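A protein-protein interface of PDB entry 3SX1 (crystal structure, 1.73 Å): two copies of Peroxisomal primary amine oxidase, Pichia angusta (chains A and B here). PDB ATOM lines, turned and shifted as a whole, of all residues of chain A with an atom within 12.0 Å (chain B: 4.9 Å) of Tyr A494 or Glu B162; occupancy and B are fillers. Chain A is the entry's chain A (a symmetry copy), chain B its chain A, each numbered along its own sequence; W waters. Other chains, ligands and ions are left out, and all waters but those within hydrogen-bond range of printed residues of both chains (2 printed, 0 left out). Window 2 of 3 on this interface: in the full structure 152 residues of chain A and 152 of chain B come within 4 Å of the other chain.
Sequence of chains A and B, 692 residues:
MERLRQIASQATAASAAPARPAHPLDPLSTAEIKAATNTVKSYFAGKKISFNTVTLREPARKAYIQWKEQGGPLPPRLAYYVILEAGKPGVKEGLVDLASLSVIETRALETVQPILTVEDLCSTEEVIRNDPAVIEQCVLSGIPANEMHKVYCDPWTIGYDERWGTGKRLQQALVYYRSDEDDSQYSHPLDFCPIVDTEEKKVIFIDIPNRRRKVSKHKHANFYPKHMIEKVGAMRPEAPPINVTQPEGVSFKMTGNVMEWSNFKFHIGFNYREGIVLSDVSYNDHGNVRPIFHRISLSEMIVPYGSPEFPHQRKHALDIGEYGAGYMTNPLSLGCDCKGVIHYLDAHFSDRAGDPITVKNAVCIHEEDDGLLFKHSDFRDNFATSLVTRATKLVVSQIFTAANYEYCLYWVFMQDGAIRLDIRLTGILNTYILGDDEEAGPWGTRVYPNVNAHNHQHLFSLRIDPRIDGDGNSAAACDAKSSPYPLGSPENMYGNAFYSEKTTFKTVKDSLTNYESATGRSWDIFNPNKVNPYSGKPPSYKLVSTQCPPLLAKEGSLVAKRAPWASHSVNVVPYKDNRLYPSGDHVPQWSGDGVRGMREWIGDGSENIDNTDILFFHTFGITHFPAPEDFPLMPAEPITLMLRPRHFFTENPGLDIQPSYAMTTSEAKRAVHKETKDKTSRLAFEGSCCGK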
ATOM      1  N   SER A 482     -17.049  -0.009 -13.545  1.00  0.00           N
ATOM      2  CA  SER A 482     -16.298  -1.213 -13.900  1.00  0.00           C
ATOM      3  C   SER A 482     -14.817  -0.889 -13.780  1.00  0.00           C
ATOM      4  O   SER A 482     -14.394   0.258 -14.018  1.00  0.00           O
ATOM      5  CB  SER A 482     -16.608  -1.652 -15.337  1.00  0.00           C
ATOM      6  OG  SER A 482     -18.004  -1.677 -15.582  1.00  0.00           O
ATOM      7  N   SER A 483     -14.008  -1.898 -13.519  1.00  0.00           N
ATOM      8  CA  SER A 483     -12.553  -1.697 -13.642  1.00  0.00           C
ATOM      9  C   SER A 483     -12.205  -1.135 -15.025  1.00  0.00           C
ATOM     10  O   SER A 483     -12.774  -1.525 -16.033  1.00  0.00           O
ATOM     11  CB  SER A 483     -11.852  -3.042 -13.451  1.00  0.00           C
ATOM     12  OG  SER A 483     -10.478  -2.896 -13.798  1.00  0.00           O
ATOM     13  N   PRO A 484     -11.178  -0.273 -15.097  1.00  0.00           N
ATOM     14  CA  PRO A 484     -10.773   0.206 -16.408  1.00  0.00           C
ATOM     15  C   PRO A 484      -9.995  -0.801 -17.236  1.00  0.00           C
ATOM     16  O   PRO A 484      -9.788  -0.562 -18.435  1.00  0.00           O
ATOM     17  CB  PRO A 484      -9.877   1.410 -16.072  1.00  0.00           C
ATOM     18  CG  PRO A 484      -9.274   1.074 -14.732  1.00  0.00           C
ATOM     19  CD  PRO A 484     -10.384   0.301 -13.989  1.00  0.00           C
ATOM     20  N   TYR A 485      -9.552  -1.897 -16.618  1.00  0.00           N
ATOM     21  CA  TYR A 485      -8.830  -2.960 -17.341  1.00  0.00           C
ATOM     22  C   TYR A 485      -9.805  -3.824 -18.118  1.00  0.00           C
ATOM     23  O   TYR A 485     -10.900  -4.129 -17.634  1.00  0.00           O
ATOM     24  CB  TYR A 485      -8.010  -3.827 -16.356  1.00  0.00           C
ATOM     25  CG  TYR A 485      -6.824  -3.082 -15.772  1.00  0.00           C
ATOM     26  CD1 TYR A 485      -6.936  -2.382 -14.586  1.00  0.00           C
ATOM     27  CD2 TYR A 485      -5.603  -3.048 -16.453  1.00  0.00           C
ATOM     28  CE1 TYR A 485      -5.874  -1.630 -14.081  1.00  0.00           C
ATOM     29  CE2 TYR A 485      -4.528  -2.307 -15.958  1.00  0.00           C
ATOM     30  CZ  TYR A 485      -4.670  -1.621 -14.765  1.00  0.00           C
ATOM     31  OH  TYR A 485      -3.620  -0.841 -14.309  1.00  0.00           O
ATOM     32  N   PRO A 486      -9.423  -4.193 -19.345  1.00  0.00           N
ATOM     33  CA  PRO A 486     -10.388  -4.826 -20.231  1.00  0.00           C
ATOM     34  C   PRO A 486     -10.614  -6.272 -19.827  1.00  0.00           C
ATOM     35  O   PRO A 486      -9.760  -6.897 -19.189  1.00  0.00           O
ATOM     36  CB  PRO A 486      -9.700  -4.785 -21.604  1.00  0.00           C
ATOM     37  CG  PRO A 486      -8.189  -4.659 -21.284  1.00  0.00           C
ATOM     38  CD  PRO A 486      -8.169  -3.810 -20.036  1.00  0.00           C
ATOM     39  N   LEU A 487     -11.729  -6.814 -20.277  1.00  0.00           N
ATOM     40  CA  LEU A 487     -11.918  -8.286 -20.321  1.00  0.00           C
ATOM     41  C   LEU A 487     -10.693  -9.004 -20.935  1.00  0.00           C
ATOM     42  O   LEU A 487     -10.098  -8.565 -21.945  1.00  0.00           O
ATOM     43  CB  LEU A 487     -13.193  -8.555 -21.141  1.00  0.00           C
ATOM     44  CG  LEU A 487     -13.529 -10.016 -21.363  1.00  0.00           C
ATOM     45  CD1 LEU A 487     -14.080 -10.635 -20.056  1.00  0.00           C
ATOM     46  CD2 LEU A 487     -14.630 -10.055 -22.442  1.00  0.00           C
ATOM     47  N   GLY A 488     -10.222 -10.038 -20.241  1.00  0.00           N
ATOM     48  CA  GLY A 488      -9.138 -10.877 -20.747  1.00  0.00           C
ATOM     49  C   GLY A 488      -7.764 -10.340 -20.377  1.00  0.00           C
ATOM     50  O   GLY A 488      -6.765 -10.960 -20.698  1.00  0.00           O
ATOM     51  N   SER A 489      -7.707  -9.269 -19.595  1.00  0.00           N
ATOM     52  CA  SER A 489      -6.408  -8.760 -19.102  1.00  0.00           C
ATOM     53  C   SER A 489      -6.046  -9.550 -17.824  1.00  0.00           C
ATOM     54  O   SER A 489      -6.925 -10.127 -17.174  1.00  0.00           O
ATOM     55  CB  SER A 489      -6.500  -7.267 -18.824  1.00  0.00           C
ATOM     56  OG  SER A 489      -7.394  -6.997 -17.752  1.00  0.00           O
ATOM     57  N   PRO A 490      -4.767  -9.570 -17.455  1.00  0.00           N
ATOM     58  CA  PRO A 490      -4.403 -10.229 -16.203  1.00  0.00           C
ATOM     59  C   PRO A 490      -5.154  -9.606 -15.007  1.00  0.00           C
ATOM     60  O   PRO A 490      -5.429 -10.310 -14.033  1.00  0.00           O
ATOM     61  CB  PRO A 490      -2.914  -9.922 -16.080  1.00  0.00           C
ATOM     62  CG  PRO A 490      -2.450  -9.923 -17.526  1.00  0.00           C
ATOM     63  CD  PRO A 490      -3.572  -9.162 -18.238  1.00  0.00           C
ATOM     64  N   GLU A 491      -5.447  -8.316 -15.101  1.00  0.00           N
ATOM     65  CA  GLU A 491      -6.077  -7.557 -14.012  1.00  0.00           C
ATOM     66  C   GLU A 491      -7.589  -7.815 -13.887  1.00  0.00           C
ATOM     67  O   GLU A 491      -8.185  -7.493 -12.848  1.00  0.00           O
ATOM     68  CB  GLU A 491      -5.888  -6.062 -14.255  1.00  0.00           C
ATOM     69  CG  GLU A 491      -4.424  -5.563 -14.140  1.00  0.00           C
ATOM     70  CD  GLU A 491      -3.609  -5.731 -15.417  1.00  0.00           C
ATOM     71  OE1 GLU A 491      -4.141  -6.209 -16.456  1.00  0.00           O
ATOM     72  OE2 GLU A 491      -2.435  -5.275 -15.402  1.00  0.00           O
ATOM     73  N   ASN A 492      -8.220  -8.268 -14.971  1.00  0.00           N
ATOM     74  CA  ASN A 492      -9.697  -8.370 -15.016  1.00  0.00           C
ATOM     75  C   ASN A 492     -10.094  -9.510 -15.955  1.00  0.00           C
ATOM     76  O   ASN A 492     -10.781  -9.305 -16.951  1.00  0.00           O
ATOM     77  CB  ASN A 492     -10.284  -7.043 -15.505  1.00  0.00           C
ATOM     78  CG  ASN A 492     -11.808  -6.935 -15.267  1.00  0.00           C
ATOM     79  OD1 ASN A 492     -12.403  -7.708 -14.507  1.00  0.00           O
ATOM     80  ND2 ASN A 492     -12.418  -5.919 -15.861  1.00  0.00           N
ATOM     81  N   MET A 493      -9.509 -10.686 -15.704  1.00  0.00           N
ATOM     82  CA  MET A 493      -9.543 -11.753 -16.679  1.00  0.00           C
ATOM     83  C   MET A 493     -10.980 -12.039 -17.177  1.00  0.00           C
ATOM     84  O   MET A 493     -11.182 -12.217 -18.382  1.00  0.00           O
ATOM     85  CB  MET A 493      -8.940 -13.029 -16.081  1.00  0.00           C
ATOM     86  CG  MET A 493      -8.957 -14.242 -17.050  1.00  0.00           C
ATOM     87  SD  MET A 493      -8.018 -13.909 -18.586  1.00  0.00           S
ATOM     88  CE  MET A 493      -6.429 -13.415 -17.928  1.00  0.00           C
ATOM     89  N   TYR A 494     -11.946 -12.142 -16.265  1.00  0.00           N
ATOM     90  CA  TYR A 494     -13.327 -12.501 -16.666  1.00  0.00           C
ATOM     91  C   TYR A 494     -14.236 -11.277 -16.737  1.00  0.00           C
ATOM     92  O   TYR A 494     -15.444 -11.393 -16.938  1.00  0.00           O
ATOM     93  CB  TYR A 494     -13.889 -13.538 -15.674  1.00  0.00           C
ATOM     94  CG  TYR A 494     -13.054 -14.797 -15.658  1.00  0.00           C
ATOM     95  CD1 TYR A 494     -11.937 -14.927 -14.797  1.00  0.00           C
ATOM     96  CD2 TYR A 494     -13.402 -15.878 -16.490  1.00  0.00           C
ATOM     97  CE1 TYR A 494     -11.198 -16.108 -14.767  1.00  0.00           C
ATOM     98  CE2 TYR A 494     -12.658 -17.062 -16.456  1.00  0.00           C
ATOM     99  CZ  TYR A 494     -11.589 -17.179 -15.554  1.00  0.00           C
ATOM    100  OH  TYR A 494     -10.831 -18.345 -15.518  1.00  0.00           O
ATOM    101  N   GLY A 495     -13.656 -10.079 -16.613  1.00  0.00           N
ATOM    102  CA  GLY A 495     -14.411  -8.871 -16.940  1.00  0.00           C
ATOM    103  C   GLY A 495     -15.390  -8.432 -15.850  1.00  0.00           C
ATOM    104  O   GLY A 495     -16.269  -7.607 -16.117  1.00  0.00           O
ATOM    105  N   ASN A 496     -15.300  -9.023 -14.650  1.00  0.00           N
ATOM    106  CA  ASN A 496     -16.295  -8.778 -13.624  1.00  0.00           C
ATOM    107  C   ASN A 496     -15.916  -7.714 -12.591  1.00  0.00           C
ATOM    108  O   ASN A 496     -16.760  -7.397 -11.718  1.00  0.00           O
ATOM    109  CB  ASN A 496     -16.629 -10.068 -12.853  1.00  0.00           C
ATOM    110  CG  ASN A 496     -15.418 -10.647 -12.143  1.00  0.00           C
ATOM    111  OD1 ASN A 496     -14.385 -10.881 -12.773  1.00  0.00           O
ATOM    112  ND2 ASN A 496     -15.518 -10.822 -10.810  1.00  0.00           N
ATOM    113  N   ALA A 497     -14.691  -7.196 -12.631  1.00  0.00           N
ATOM    114  CA  ALA A 497     -14.227  -6.342 -11.505  1.00  0.00           C
ATOM    115  C   ALA A 497     -14.966  -5.004 -11.500  1.00  0.00           C
ATOM    116  O   ALA A 497     -15.180  -4.403 -12.543  1.00  0.00           O
ATOM    117  CB  ALA A 497     -12.703  -6.089 -11.606  1.00  0.00           C
ATOM    118  N   PHE A 498     -15.316  -4.523 -10.322  1.00  0.00           N
ATOM    119  CA  PHE A 498     -15.953  -3.203 -10.237  1.00  0.00           C
ATOM    120  C   PHE A 498     -15.725  -2.636  -8.838  1.00  0.00           C
ATOM    121  O   PHE A 498     -15.463  -3.377  -7.898  1.00  0.00           O
ATOM    122  CB  PHE A 498     -17.458  -3.195 -10.639  1.00  0.00           C
ATOM    123  CG  PHE A 498     -18.384  -3.813  -9.627  1.00  0.00           C
ATOM    124  CD1 PHE A 498     -18.816  -3.077  -8.530  1.00  0.00           C
ATOM    125  CD2 PHE A 498     -18.850  -5.117  -9.797  1.00  0.00           C
ATOM    126  CE1 PHE A 498     -19.752  -3.636  -7.631  1.00  0.00           C
ATOM    127  CE2 PHE A 498     -19.796  -5.685  -8.898  1.00  0.00           C
ATOM    128  CZ  PHE A 498     -20.196  -4.964  -7.803  1.00  0.00           C
ATOM    129  N   TYR B 160     -19.933 -21.350 -13.519  1.00  0.00           N
ATOM    130  CA  TYR B 160     -19.319 -21.862 -14.750  1.00  0.00           C
ATOM    131  C   TYR B 160     -17.819 -21.925 -14.584  1.00  0.00           C
ATOM    132  O   TYR B 160     -17.178 -20.958 -14.126  1.00  0.00           O
ATOM    133  CB  TYR B 160     -19.629 -20.951 -15.940  1.00  0.00           C
ATOM    134  CG  TYR B 160     -18.947 -21.462 -17.180  1.00  0.00           C
ATOM    135  CD1 TYR B 160     -19.399 -22.629 -17.823  1.00  0.00           C
ATOM    136  CD2 TYR B 160     -17.871 -20.766 -17.729  1.00  0.00           C
ATOM    137  CE1 TYR B 160     -18.761 -23.103 -18.965  1.00  0.00           C
ATOM    138  CE2 TYR B 160     -17.190 -21.271 -18.861  1.00  0.00           C
ATOM    139  CZ  TYR B 160     -17.680 -22.397 -19.482  1.00  0.00           C
ATOM    140  OH  TYR B 160     -17.085 -22.851 -20.627  1.00  0.00           O
ATOM    141  N   ASP B 161     -17.263 -23.083 -14.935  1.00  0.00           N
ATOM    142  CA  ASP B 161     -15.807 -23.236 -14.904  1.00  0.00           C
ATOM    143  C   ASP B 161     -15.428 -23.861 -16.232  1.00  0.00           C
ATOM    144  O   ASP B 161     -15.822 -24.991 -16.509  1.00  0.00           O
ATOM    145  CB  ASP B 161     -15.409 -24.189 -13.762  1.00  0.00           C
ATOM    146  CG  ASP B 161     -13.910 -24.191 -13.511  1.00  0.00           C
ATOM    147  OD1 ASP B 161     -13.128 -24.260 -14.486  1.00  0.00           O
ATOM    148  OD2 ASP B 161     -13.509 -23.837 -12.383  1.00  0.00           O
ATOM    149  N   GLU B 162     -14.605 -23.145 -17.007  1.00  0.00           N
ATOM    150  CA  GLU B 162     -14.233 -23.575 -18.360  1.00  0.00           C
ATOM    151  C   GLU B 162     -13.355 -24.811 -18.353  1.00  0.00           C
ATOM    152  O   GLU B 162     -13.030 -25.349 -19.418  1.00  0.00           O
ATOM    153  CB  GLU B 162     -13.521 -22.423 -19.109  1.00  0.00           C
ATOM    154  CG  GLU B 162     -12.196 -21.952 -18.521  1.00  0.00           C
ATOM    155  CD  GLU B 162     -12.320 -20.950 -17.348  1.00  0.00           C
ATOM    156  OE1 GLU B 162     -13.427 -20.708 -16.801  1.00  0.00           O
ATOM    157  OE2 GLU B 162     -11.251 -20.443 -16.930  1.00  0.00           O
ATOM    158  N   ARG B 163     -12.887 -25.228 -17.171  1.00  0.00           N
ATOM    159  CA  ARG B 163     -12.138 -26.507 -17.140  1.00  0.00           C
ATOM    160  C   ARG B 163     -13.031 -27.728 -17.300  1.00  0.00           C
ATOM    161  O   ARG B 163     -12.553 -28.776 -17.725  1.00  0.00           O
ATOM    162  CB  ARG B 163     -11.336 -26.615 -15.841  1.00  0.00           C
ATOM    163  CG  ARG B 163     -10.223 -25.567 -15.818  1.00  0.00           C
ATOM    164  CD  ARG B 163      -9.540 -25.478 -14.434  1.00  0.00           C
ATOM    165  NE  ARG B 163     -10.469 -25.000 -13.420  1.00  0.00           N
ATOM    166  CZ  ARG B 163     -10.149 -24.824 -12.136  1.00  0.00           C
ATOM    167  NH1 ARG B 163      -8.890 -25.032 -11.733  1.00  0.00           N
ATOM    168  NH2 ARG B 163     -11.083 -24.437 -11.261  1.00  0.00           N
ATOM    169  N   TRP B 164     -14.330 -27.593 -17.019  1.00  0.00           N
ATOM    170  CA  TRP B 164     -15.219 -28.779 -17.044  1.00  0.00           C
ATOM    171  C   TRP B 164     -16.515 -28.599 -17.843  1.00  0.00           C
ATOM    172  O   TRP B 164     -17.168 -29.596 -18.167  1.00  0.00           O
ATOM    173  CB  TRP B 164     -15.615 -29.277 -15.642  1.00  0.00           C
ATOM    174  CG  TRP B 164     -14.434 -29.820 -14.869  1.00  0.00           C
ATOM    175  CD1 TRP B 164     -13.771 -30.999 -15.081  1.00  0.00           C
ATOM    176  CD2 TRP B 164     -13.668 -29.080 -13.917  1.00  0.00           C
ATOM    177  NE1 TRP B 164     -12.659 -31.065 -14.250  1.00  0.00           N
ATOM    178  CE2 TRP B 164     -12.564 -29.887 -13.550  1.00  0.00           C
ATOM    179  CE3 TRP B 164     -13.823 -27.813 -13.322  1.00  0.00           C
ATOM    180  CZ2 TRP B 164     -11.625 -29.475 -12.569  1.00  0.00           C
ATOM    181  CZ3 TRP B 164     -12.919 -27.407 -12.340  1.00  0.00           C
ATOM    182  CH2 TRP B 164     -11.805 -28.236 -11.998  1.00  0.00           C
ATOM    183  N   GLY B 165     -16.874 -27.365 -18.196  1.00  0.00           N
ATOM    184  CA  GLY B 165     -18.103 -27.143 -18.957  1.00  0.00           C
ATOM    185  C   GLY B 165     -19.296 -27.735 -18.203  1.00  0.00           C
ATOM    186  O   GLY B 165     -19.438 -27.544 -16.977  1.00  0.00           O
ATOM    187  N   PHE B 310      -8.899 -14.907  -8.999  1.00  0.00           N
ATOM    188  CA  PHE B 310      -9.368 -16.283  -9.137  1.00  0.00           C
ATOM    189  C   PHE B 310      -9.509 -16.872  -7.730  1.00  0.00           C
ATOM    190  O   PHE B 310      -8.647 -16.611  -6.848  1.00  0.00           O
ATOM    191  CB  PHE B 310      -8.328 -17.053  -9.946  1.00  0.00           C
ATOM    192  CG  PHE B 310      -8.784 -18.382 -10.430  1.00  0.00           C
ATOM    193  CD1 PHE B 310      -9.425 -18.492 -11.659  1.00  0.00           C
ATOM    194  CD2 PHE B 310      -8.564 -19.538  -9.680  1.00  0.00           C
ATOM    195  CE1 PHE B 310      -9.869 -19.729 -12.148  1.00  0.00           C
ATOM    196  CE2 PHE B 310      -9.080 -20.780 -10.154  1.00  0.00           C
ATOM    197  CZ  PHE B 310      -9.700 -20.855 -11.392  1.00  0.00           C
ATOM    198  N   GLN B 313     -14.386 -15.087  -9.754  1.00  0.00           N
ATOM    199  CA  GLN B 313     -15.273 -14.907 -10.921  1.00  0.00           C
ATOM    200  C   GLN B 313     -16.449 -15.886 -10.939  1.00  0.00           C
ATOM    201  O   GLN B 313     -17.403 -15.688 -11.691  1.00  0.00           O
ATOM    202  CB  GLN B 313     -14.502 -14.968 -12.260  1.00  0.00           C
ATOM    203  CG  GLN B 313     -14.207 -16.434 -12.756  1.00  0.00           C
ATOM    204  CD  GLN B 313     -13.044 -17.124 -12.039  1.00  0.00           C
ATOM    205  OE1 GLN B 313     -12.359 -16.531 -11.181  1.00  0.00           O
ATOM    206  NE2 GLN B 313     -12.834 -18.419 -12.373  1.00  0.00           N
ATOM    207  N   SER B 557     -18.179 -10.751 -20.764  1.00  0.00           N
ATOM    208  CA  SER B 557     -17.880 -11.419 -19.509  1.00  0.00           C
ATOM    209  C   SER B 557     -18.759 -12.653 -19.299  1.00  0.00           C
ATOM    210  O   SER B 557     -19.810 -12.746 -19.883  1.00  0.00           O
ATOM    211  CB  SER B 557     -18.047 -10.485 -18.316  1.00  0.00           C
ATOM    212  OG  SER B 557     -19.385 -10.036 -18.226  1.00  0.00           O
ATOM    213  N   LEU B 558     -18.322 -13.564 -18.450  1.00  0.00           N
ATOM    214  CA  LEU B 558     -19.127 -14.689 -18.055  1.00  0.00           C
ATOM    215  C   LEU B 558     -20.514 -14.234 -17.568  1.00  0.00           C
ATOM    216  O   LEU B 558     -21.539 -14.798 -17.932  1.00  0.00           O
ATOM    217  CB  LEU B 558     -18.367 -15.409 -16.952  1.00  0.00           C
ATOM    218  CG  LEU B 558     -18.846 -16.772 -16.560  1.00  0.00           C
ATOM    219  CD1 LEU B 558     -19.136 -17.610 -17.830  1.00  0.00           C
ATOM    220  CD2 LEU B 558     -17.749 -17.439 -15.679  1.00  0.00           C
HETATM  221  O   HOH W   1     -17.684 -12.394 -15.495  1.00  0.00           O
HETATM  222  O   HOH W   2     -15.401 -14.114 -19.040  1.00  0.00           O
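OE2 of Glu B162 is in hydrogen-bond range of OH of Tyr A494 (2.6 Å).
Leu A487 touches Ser B557.
CE1 of Phe B310 touches OH of Tyr A494, 3.8 Å away.
CD1 of Tyr A494 touches CG of Gln B313, 3.4 Å away.
Ser B557 touches Tyr A494 (CB to O, 3.1 Å).
Tyr A494 touches Leu B558.
Pro A486 touches none of the printed residues of chain B.
Of the printed residues of chain B, Leu A487 touches Ser B557 (3.9 Å).
No residue of chain A comes within 4 Å of Tyr B160.
Of chain A, only Tyr A494 (2.6 Å) comes within 4 Å of Glu B162.
No residue of chain A comes within 4 Å of Arg B163.
No residue of chain A comes within 4 Å of Trp B164.
No residue of chain A comes within 4 Å of Gly B165.
Printed residues of chain A within 4 Å of Phe B310: Tyr A494 (3.8 Å).
Printed residues of chain A within 4 Å of Leu B558: Tyr A494.
The nearest printed residue of chain B that does not touch Tyr A494 is Tyr B160 (6.4 Å).
Of the 10 printed residues of chain B, 5 touch a printed residue of chain A.
Printed residues of chain B that touch a printed residue of chain A: Glu B162, Phe B310, Gln B313, Ser B557 and Leu B558.
Hydrophobic or aromatic side chains of chain B that line the printed part of chain A: Phe B310.
Hydrophobic or aromatic side chains of chain A that line the printed part of chain B: Leu A487 and Tyr A494.
Among the printed residues, 6 pairs touch across the chains.
Among the printed residues, no Asp or Glu carboxylate lies within 4 Å of a Lys or Arg side-chain nitrogen of the other chain.
No position is printed for both chains.
Of the 6 pairs that touch across the chains among the printed residues, none has its exchanged pair printed and touching as well.
Water W1 lies within hydrogen-bond range of O of Tyr A494 (2.8 Å) and N of Leu B558 (3.2 Å).
Water W2 bridges N of Leu B558 and O of Tyr A494.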
